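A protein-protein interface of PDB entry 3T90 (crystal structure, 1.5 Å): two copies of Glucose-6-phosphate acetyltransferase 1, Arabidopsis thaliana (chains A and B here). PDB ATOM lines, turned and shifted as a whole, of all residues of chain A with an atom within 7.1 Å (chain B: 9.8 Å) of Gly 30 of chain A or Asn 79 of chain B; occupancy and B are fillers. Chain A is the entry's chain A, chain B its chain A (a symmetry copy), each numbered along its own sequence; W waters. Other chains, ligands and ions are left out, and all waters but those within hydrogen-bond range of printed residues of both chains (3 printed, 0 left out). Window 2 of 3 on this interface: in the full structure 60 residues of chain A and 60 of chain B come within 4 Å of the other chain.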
ATOM      1  N   ILE A  20      13.522  20.329 -17.272  1.00  0.00           N
ATOM      2  CA  ILE A  20      14.126  19.023 -17.156  1.00  0.00           C
ATOM      3  C   ILE A  20      13.700  18.154 -18.360  1.00  0.00           C
ATOM      4  O   ILE A  20      14.550  17.475 -18.974  1.00  0.00           O
ATOM      5  CB  ILE A  20      13.702  18.362 -15.824  1.00  0.00           C
ATOM      6  CG1 ILE A  20      14.171  19.260 -14.644  1.00  0.00           C
ATOM      7  CG2 ILE A  20      14.238  16.874 -15.707  1.00  0.00           C
ATOM      8  CD1 ILE A  20      15.745  19.327 -14.585  1.00  0.00           C
ATOM      9  N   GLY A  24      16.167  16.240 -21.243  1.00  0.00           N
ATOM     10  CA  GLY A  24      16.015  14.836 -21.613  1.00  0.00           C
ATOM     11  C   GLY A  24      16.181  14.610 -23.128  1.00  0.00           C
ATOM     12  O   GLY A  24      16.415  13.477 -23.521  1.00  0.00           O
ATOM     13  N   THR A  27      20.354  14.164 -22.840  1.00  0.00           N
ATOM     14  CA  THR A  27      20.672  12.816 -22.312  1.00  0.00           C
ATOM     15  C   THR A  27      19.776  12.550 -21.105  1.00  0.00           C
ATOM     16  O   THR A  27      18.875  13.353 -20.779  1.00  0.00           O
ATOM     17  CB  THR A  27      22.140  12.710 -22.003  1.00  0.00           C
ATOM     18  OG1 THR A  27      22.471  11.306 -21.855  1.00  0.00           O
ATOM     19  CG2 THR A  27      22.582  13.436 -20.688  1.00  0.00           C
ATOM     20  N   VAL A  28      20.015  11.426 -20.455  1.00  0.00           N
ATOM     21  CA  VAL A  28      19.206  10.939 -19.352  1.00  0.00           C
ATOM     22  C   VAL A  28      19.167  12.010 -18.250  1.00  0.00           C
ATOM     23  O   VAL A  28      20.214  12.520 -17.823  1.00  0.00           O
ATOM     24  CB  VAL A  28      19.878   9.681 -18.769  1.00  0.00           C
ATOM     25  CG1 VAL A  28      19.146   9.190 -17.486  1.00  0.00           C
ATOM     26  CG2 VAL A  28      20.031   8.598 -19.832  1.00  0.00           C
ATOM     27  N   THR A  29      17.952  12.305 -17.784  1.00  0.00           N
ATOM     28  CA  THR A  29      17.799  13.161 -16.605  1.00  0.00           C
ATOM     29  C   THR A  29      17.390  12.415 -15.366  1.00  0.00           C
ATOM     30  O   THR A  29      17.690  12.862 -14.233  1.00  0.00           O
ATOM     31  CB  THR A  29      16.750  14.316 -16.787  1.00  0.00           C
ATOM     32  OG1 THR A  29      15.455  13.736 -17.059  1.00  0.00           O
ATOM     33  CG2 THR A  29      17.098  15.189 -18.023  1.00  0.00           C
ATOM     34  N   GLY A  30      16.694  11.319 -15.546  1.00  0.00           N
ATOM     35  CA  GLY A  30      15.898  10.764 -14.431  1.00  0.00           C
ATOM     36  C   GLY A  30      14.675  11.661 -14.150  1.00  0.00           C
ATOM     37  O   GLY A  30      14.435  12.714 -14.722  1.00  0.00           O
ATOM     38  N   SER A  31      13.893  11.266 -13.147  1.00  0.00           N
ATOM     39  CA  SER A  31      12.637  12.008 -12.870  1.00  0.00           C
ATOM     40  C   SER A  31      12.895  12.949 -11.683  1.00  0.00           C
ATOM     41  O   SER A  31      12.550  12.664 -10.509  1.00  0.00           O
ATOM     42  CB  SER A  31      11.410  11.098 -12.583  1.00  0.00           C
ATOM     43  OG  SER A  31      11.162  10.172 -13.654  1.00  0.00           O
ATOM     44  N   VAL A  32      13.490  14.117 -11.961  1.00  0.00           N
ATOM     45  CA  VAL A  32      14.012  15.052 -10.950  1.00  0.00           C
ATOM     46  C   VAL A  32      12.826  15.696 -10.185  1.00  0.00           C
ATOM     47  O   VAL A  32      11.949  16.316 -10.746  1.00  0.00           O
ATOM     48  CB  VAL A  32      14.845  16.188 -11.662  1.00  0.00           C
ATOM     49  CG1 VAL A  32      15.297  17.263 -10.674  1.00  0.00           C
ATOM     50  CG2 VAL A  32      16.082  15.579 -12.399  1.00  0.00           C
ATOM     51  N   THR A  33      12.820  15.536  -8.898  1.00  0.00           N
ATOM     52  CA  THR A  33      11.761  16.067  -8.063  1.00  0.00           C
ATOM     53  C   THR A  33      11.882  17.579  -7.911  1.00  0.00           C
ATOM     54  O   THR A  33      12.962  18.151  -8.122  1.00  0.00           O
ATOM     55  CB  THR A  33      11.758  15.442  -6.653  1.00  0.00           C
ATOM     56  OG1 THR A  33      12.965  15.817  -5.998  1.00  0.00           O
ATOM     57  CG2 THR A  33      11.659  13.898  -6.699  1.00  0.00           C
ATOM     58  N   GLU A  36      14.652  18.262  -5.319  1.00  0.00           N
ATOM     59  CA  GLU A  36      15.976  18.133  -5.877  1.00  0.00           C
ATOM     60  C   GLU A  36      16.296  19.265  -6.859  1.00  0.00           C
ATOM     61  O   GLU A  36      17.391  19.827  -6.806  1.00  0.00           O
ATOM     62  CB  GLU A  36      16.119  16.786  -6.578  1.00  0.00           C
ATOM     63  CG  GLU A  36      17.550  16.580  -6.971  1.00  0.00           C
ATOM     64  CD  GLU A  36      18.548  16.042  -5.909  1.00  0.00           C
ATOM     65  OE1 GLU A  36      18.429  16.287  -4.666  1.00  0.00           O
ATOM     66  OE2 GLU A  36      19.504  15.363  -6.363  1.00  0.00           O
ATOM     67  N   ARG A  39      17.148  22.227  -4.769  1.00  0.00           N
ATOM     68  CA  ARG A  39      18.418  22.054  -4.073  1.00  0.00           C
ATOM     69  C   ARG A  39      19.511  22.407  -5.064  1.00  0.00           C
ATOM     70  O   ARG A  39      20.447  23.156  -4.699  1.00  0.00           O
ATOM     71  CB  ARG A  39      18.564  20.597  -3.634  1.00  0.00           C
ATOM     72  CG  ARG A  39      19.760  20.377  -2.748  1.00  0.00           C
ATOM     73  CD  ARG A  39      19.958  18.940  -2.296  1.00  0.00           C
ATOM     74  NE  ARG A  39      20.241  18.092  -3.458  1.00  0.00           N
ATOM     75  CZ  ARG A  39      21.461  17.865  -3.921  1.00  0.00           C
ATOM     76  NH1 ARG A  39      22.501  18.344  -3.254  1.00  0.00           N
ATOM     77  NH2 ARG A  39      21.640  17.145  -5.030  1.00  0.00           N
ATOM     78  N   ARG A  40      19.457  21.830  -6.270  1.00  0.00           N
ATOM     79  CA  ARG A  40      20.560  21.982  -7.215  1.00  0.00           C
ATOM     80  C   ARG A  40      20.531  23.381  -7.815  1.00  0.00           C
ATOM     81  O   ARG A  40      21.589  23.979  -8.045  1.00  0.00           O
ATOM     82  CB  ARG A  40      20.387  20.868  -8.282  1.00  0.00           C
ATOM     83  CG  ARG A  40      21.463  20.918  -9.501  1.00  0.00           C
ATOM     84  CD  ARG A  40      22.917  21.119  -9.064  1.00  0.00           C
ATOM     85  NE  ARG A  40      23.296  20.251  -7.952  1.00  0.00           N
ATOM     86  CZ  ARG A  40      23.863  19.077  -8.134  1.00  0.00           C
ATOM     87  NH1 ARG A  40      24.033  18.533  -9.373  1.00  0.00           N
ATOM     88  NH2 ARG A  40      24.335  18.457  -7.075  1.00  0.00           N
ATOM     89  N   LYS B  74      28.373  20.736 -11.215  1.00  0.00           N
ATOM     90  CA  LYS B  74      27.030  20.226 -10.874  1.00  0.00           C
ATOM     91  C   LYS B  74      26.063  20.516 -11.984  1.00  0.00           C
ATOM     92  O   LYS B  74      26.022  21.628 -12.505  1.00  0.00           O
ATOM     93  CB  LYS B  74      26.564  20.900  -9.621  1.00  0.00           C
ATOM     94  CG  LYS B  74      27.439  20.496  -8.386  1.00  0.00           C
ATOM     95  CD  LYS B  74      26.957  21.165  -7.123  1.00  0.00           C
ATOM     96  CE  LYS B  74      27.925  20.754  -6.013  1.00  0.00           C
ATOM     97  NZ  LYS B  74      29.063  21.761  -5.943  1.00  0.00           N
ATOM     98  N   LYS B  75      25.231  19.520 -12.322  1.00  0.00           N
ATOM     99  CA  LYS B  75      24.252  19.627 -13.416  1.00  0.00           C
ATOM    100  C   LYS B  75      22.863  19.327 -12.949  1.00  0.00           C
ATOM    101  O   LYS B  75      22.705  18.875 -11.764  1.00  0.00           O
ATOM    102  CB  LYS B  75      24.617  18.604 -14.507  1.00  0.00           C
ATOM    103  CG  LYS B  75      25.981  18.854 -15.157  1.00  0.00           C
ATOM    104  CD  LYS B  75      26.144  17.835 -16.265  1.00  0.00           C
ATOM    105  CE  LYS B  75      27.391  17.994 -17.137  1.00  0.00           C
ATOM    106  NZ  LYS B  75      27.295  19.224 -18.019  1.00  0.00           N
ATOM    107  N   PHE B  76      21.852  19.511 -13.798  1.00  0.00           N
ATOM    108  CA  PHE B  76      20.512  19.000 -13.519  1.00  0.00           C
ATOM    109  C   PHE B  76      20.288  17.654 -14.153  1.00  0.00           C
ATOM    110  O   PHE B  76      19.583  16.810 -13.608  1.00  0.00           O
ATOM    111  CB  PHE B  76      19.410  19.990 -14.031  1.00  0.00           C
ATOM    112  CG  PHE B  76      19.299  21.250 -13.221  1.00  0.00           C
ATOM    113  CD1 PHE B  76      18.472  21.304 -12.095  1.00  0.00           C
ATOM    114  CD2 PHE B  76      19.985  22.360 -13.570  1.00  0.00           C
ATOM    115  CE1 PHE B  76      18.415  22.463 -11.350  1.00  0.00           C
ATOM    116  CE2 PHE B  76      19.911  23.514 -12.810  1.00  0.00           C
ATOM    117  CZ  PHE B  76      19.091  23.558 -11.712  1.00  0.00           C
ATOM    118  N   LEU B  77      20.880  17.409 -15.293  1.00  0.00           N
ATOM    119  CA  LEU B  77      20.713  16.077 -15.931  1.00  0.00           C
ATOM    120  C   LEU B  77      21.463  15.001 -15.128  1.00  0.00           C
ATOM    121  O   LEU B  77      22.205  15.228 -14.142  1.00  0.00           O
ATOM    122  CB  LEU B  77      20.913  16.154 -17.469  1.00  0.00           C
ATOM    123  CG  LEU B  77      22.319  16.556 -17.896  1.00  0.00           C
ATOM    124  CD1 LEU B  77      23.395  15.446 -17.684  1.00  0.00           C
ATOM    125  CD2 LEU B  77      22.319  17.085 -19.263  1.00  0.00           C
ATOM    126  N   ARG B  78      21.203  13.716 -15.465  1.00  0.00           N
ATOM    127  CA  ARG B  78      21.815  12.640 -14.723  1.00  0.00           C
ATOM    128  C   ARG B  78      21.433  12.679 -13.225  1.00  0.00           C
ATOM    129  O   ARG B  78      22.209  12.459 -12.355  1.00  0.00           O
ATOM    130  CB  ARG B  78      23.364  12.510 -14.967  1.00  0.00           C
ATOM    131  CG  ARG B  78      23.691  11.877 -16.341  1.00  0.00           C
ATOM    132  CD  ARG B  78      23.610  10.328 -16.108  1.00  0.00           C
ATOM    133  NE  ARG B  78      24.303   9.533 -17.142  1.00  0.00           N
ATOM    134  CZ  ARG B  78      24.960   8.429 -16.860  1.00  0.00           C
ATOM    135  NH1 ARG B  78      24.992   7.958 -15.546  1.00  0.00           N
ATOM    136  NH2 ARG B  78      25.551   7.756 -17.876  1.00  0.00           N
ATOM    137  N   ASN B  79      20.116  12.934 -12.984  1.00  0.00           N
ATOM    138  CA  ASN B  79      19.584  12.977 -11.614  1.00  0.00           C
ATOM    139  C   ASN B  79      20.323  13.965 -10.772  1.00  0.00           C
ATOM    140  O   ASN B  79      20.805  13.684  -9.699  1.00  0.00           O
ATOM    141  CB  ASN B  79      19.579  11.551 -10.988  1.00  0.00           C
ATOM    142  CG  ASN B  79      18.450  10.695 -11.530  1.00  0.00           C
ATOM    143  OD1 ASN B  79      17.336  10.778 -11.033  1.00  0.00           O
ATOM    144  ND2 ASN B  79      18.743   9.873 -12.548  1.00  0.00           N
ATOM    145  N   CYS B  80      20.420  15.175 -11.304  1.00  0.00           N
ATOM    146  CA  CYS B  80      21.229  16.238 -10.598  1.00  0.00           C
ATOM    147  C   CYS B  80      22.652  15.670 -10.306  1.00  0.00           C
ATOM    148  O   CYS B  80      23.174  15.687  -9.161  1.00  0.00           O
ATOM    149  CB  CYS B  80      20.541  16.808  -9.352  1.00  0.00           C
ATOM    150  SG  CYS B  80      19.044  17.738  -9.856  1.00  0.00           S
ATOM    151  N   GLY B  81      23.269  15.194 -11.394  1.00  0.00           N
ATOM    152  CA  GLY B  81      24.600  14.604 -11.315  1.00  0.00           C
ATOM    153  C   GLY B  81      25.729  15.610 -11.324  1.00  0.00           C
ATOM    154  O   GLY B  81      25.519  16.803 -11.381  1.00  0.00           O
ATOM    155  N   LYS B  82      26.931  15.034 -11.308  1.00  0.00           N
ATOM    156  CA  LYS B  82      28.191  15.797 -11.246  1.00  0.00           C
ATOM    157  C   LYS B  82      29.152  15.233 -12.219  1.00  0.00           C
ATOM    158  O   LYS B  82      29.297  13.993 -12.336  1.00  0.00           O
ATOM    159  CB  LYS B  82      28.815  15.746  -9.824  1.00  0.00           C
ATOM    160  CG  LYS B  82      28.036  16.500  -8.827  1.00  0.00           C
ATOM    161  CD  LYS B  82      28.873  16.626  -7.578  1.00  0.00           C
ATOM    162  CE  LYS B  82      29.159  15.334  -6.936  1.00  0.00           C
ATOM    163  NZ  LYS B  82      29.264  15.613  -5.386  1.00  0.00           N
ATOM    164  N   GLY B 116      31.256  10.980  -6.253  1.00  0.00           N
ATOM    165  CA  GLY B 116      29.990  10.595  -6.853  1.00  0.00           C
ATOM    166  C   GLY B 116      29.733  11.181  -8.219  1.00  0.00           C
ATOM    167  O   GLY B 116      28.596  11.246  -8.653  1.00  0.00           O
ATOM    168  N   TYR B 118      29.338  11.090 -12.269  1.00  0.00           N
ATOM    169  CA  TYR B 118      28.948   9.966 -13.176  1.00  0.00           C
ATOM    170  C   TYR B 118      29.949   9.811 -14.351  1.00  0.00           C
ATOM    171  O   TYR B 118      29.947   8.773 -15.020  1.00  0.00           O
ATOM    172  CB  TYR B 118      27.509  10.184 -13.692  1.00  0.00           C
ATOM    173  CG  TYR B 118      27.328  11.379 -14.629  1.00  0.00           C
ATOM    174  CD1 TYR B 118      27.453  11.245 -15.985  1.00  0.00           C
ATOM    175  CD2 TYR B 118      27.079  12.612 -14.106  1.00  0.00           C
ATOM    176  CE1 TYR B 118      27.294  12.378 -16.848  1.00  0.00           C
ATOM    177  CE2 TYR B 118      26.934  13.710 -14.911  1.00  0.00           C
ATOM    178  CZ  TYR B 118      27.000  13.590 -16.278  1.00  0.00           C
ATOM    179  OH  TYR B 118      26.890  14.730 -17.094  1.00  0.00           O
HETATM  180  O   HOH W   1      15.081  11.559  -9.197  1.00  0.00           O
HETATM  181  O   HOH W   2      25.260  15.619  -7.398  1.00  0.00           O
HETATM  182  O   HOH W   3      19.370  13.140  -7.388  1.00  0.00           O
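The backbone carbonyl oxygen (O) of Val 28 of chain A is in hydrogen-bond range of the backbone NH (N) of Arg 78 of chain B (2.8 Å). The guanidinium group (NH1) of Arg 40 of chain A is in hydrogen-bond range of the backbone carbonyl oxygen (O) of Lys 75 of chain B, 2.8 Å away. The backbone carbonyl oxygen of Thr 29 of chain A sits at hydrogen-bond distance from the backbone NH of Asn 79 of chain B (2.7 Å). NH1 of Arg 40 of chain A is in hydrogen-bond range of O of Cys 80 of chain B (3.0 Å). NH1 of Arg 40 of chain A is in hydrogen-bond range of O of Gly 81 of chain B (3.0 Å).
The side-chain hydroxyl of Thr 33 of chain A lies within hydrogen-bond range of the backbone NH of Glu 36 of chain A. NE of Arg 39 of chain A lies within salt-bridge range of OE1 of Glu 36 of chain A (2.8 Å). The backbone NH (N) of Lys 75 of chain B sits at hydrogen-bond distance from the backbone carbonyl oxygen (O) of Gly 81 of chain B, at 2.9 Å.
CD1 of Ile 20 of chain A touches CB of Phe 76 of chain B, at 3.8 Å. Leu 77 of chain B touches Thr 27 of chain A (CD1 to CG2, 3.7 Å). Val 28 of chain A touches Leu 77 of chain B (O to CB, 3.7 Å). CB of Leu 77 of chain B touches CG2 of Thr 29 of chain A (3.97 Å). CA of Thr 29 of chain A touches N of Arg 78 of chain B, at 3.6 Å. Val 32 of chain A touches Phe 76 of chain B. Val 32 of chain A touches Cys 80 of chain B (CG1 to SG, 3.9 Å). SG of Cys 80 of chain B touches CG of Glu 36 of chain A (3.4 Å). NH1 of Arg 40 of chain A touches CB of Lys 74 of chain B (3.5 Å). Phe 76 of chain B touches Arg 40 of chain A.
Of chain B, only Asn 79 comes within 4 Å of Gly 30 of chain A. Asn 79 of chain B touches just these residues of chain A: Thr 29, Gly 30 and Glu 36. Thr 29 of chain A touches just these residues of chain B: Leu 77, Arg 78 and Asn 79. No residue of chain B comes within 4 Å of Ser 31 of chain A. Printed residues of chain A within 4 Å of Cys 80 of chain B: Val 32, Glu 36 and Arg 40. Of the printed residues of chain A, Phe 76 of chain B touches Ile 20 (3.8 Å), Val 32 (3.9 Å) and Arg 40 (3.9 Å). Of the printed residues of chain A, Gly 81 of chain B touches Arg 40. Of the printed residues of chain A, Arg 78 of chain B touches Val 28 (2.8 Å) and Thr 29 (3.6 Å). Of the printed residues of chain A, Leu 77 of chain B touches Thr 27 (3.7 Å), Val 28 (3.7 Å) and Thr 29 (3.97 Å). Thr 33 of chain A touches none of the printed residues of chain B. The nearest residue of chain B that does not touch Gly 30 of chain A is Arg 78 of chain B (5.1 Å).
Hydrophobic or aromatic side chains of chain B that line the printed part of chain A: Phe 76 and Leu 77.
No position is printed for both chains.
Water W3 bridges the side-chain carboxylate of Glu 36 of chain A (2.5 Å) and the backbone carbonyl oxygen of Asn 79 of chain B (2.8 Å). Water W2 lies within hydrogen-bond range of the backbone carbonyl oxygen (O) of Cys 80 of chain B (2.7 Å) and the guanidinium group (NH2) of Arg 40 of chain A (3.0 Å). Water W1 lies within hydrogen-bond range of the side-chain amide oxygen (OD1) of Asn 79 of chain B (3.0 Å) and the backbone carbonyl oxygen (O) of Ser 31 of chain A (3.1 Å).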
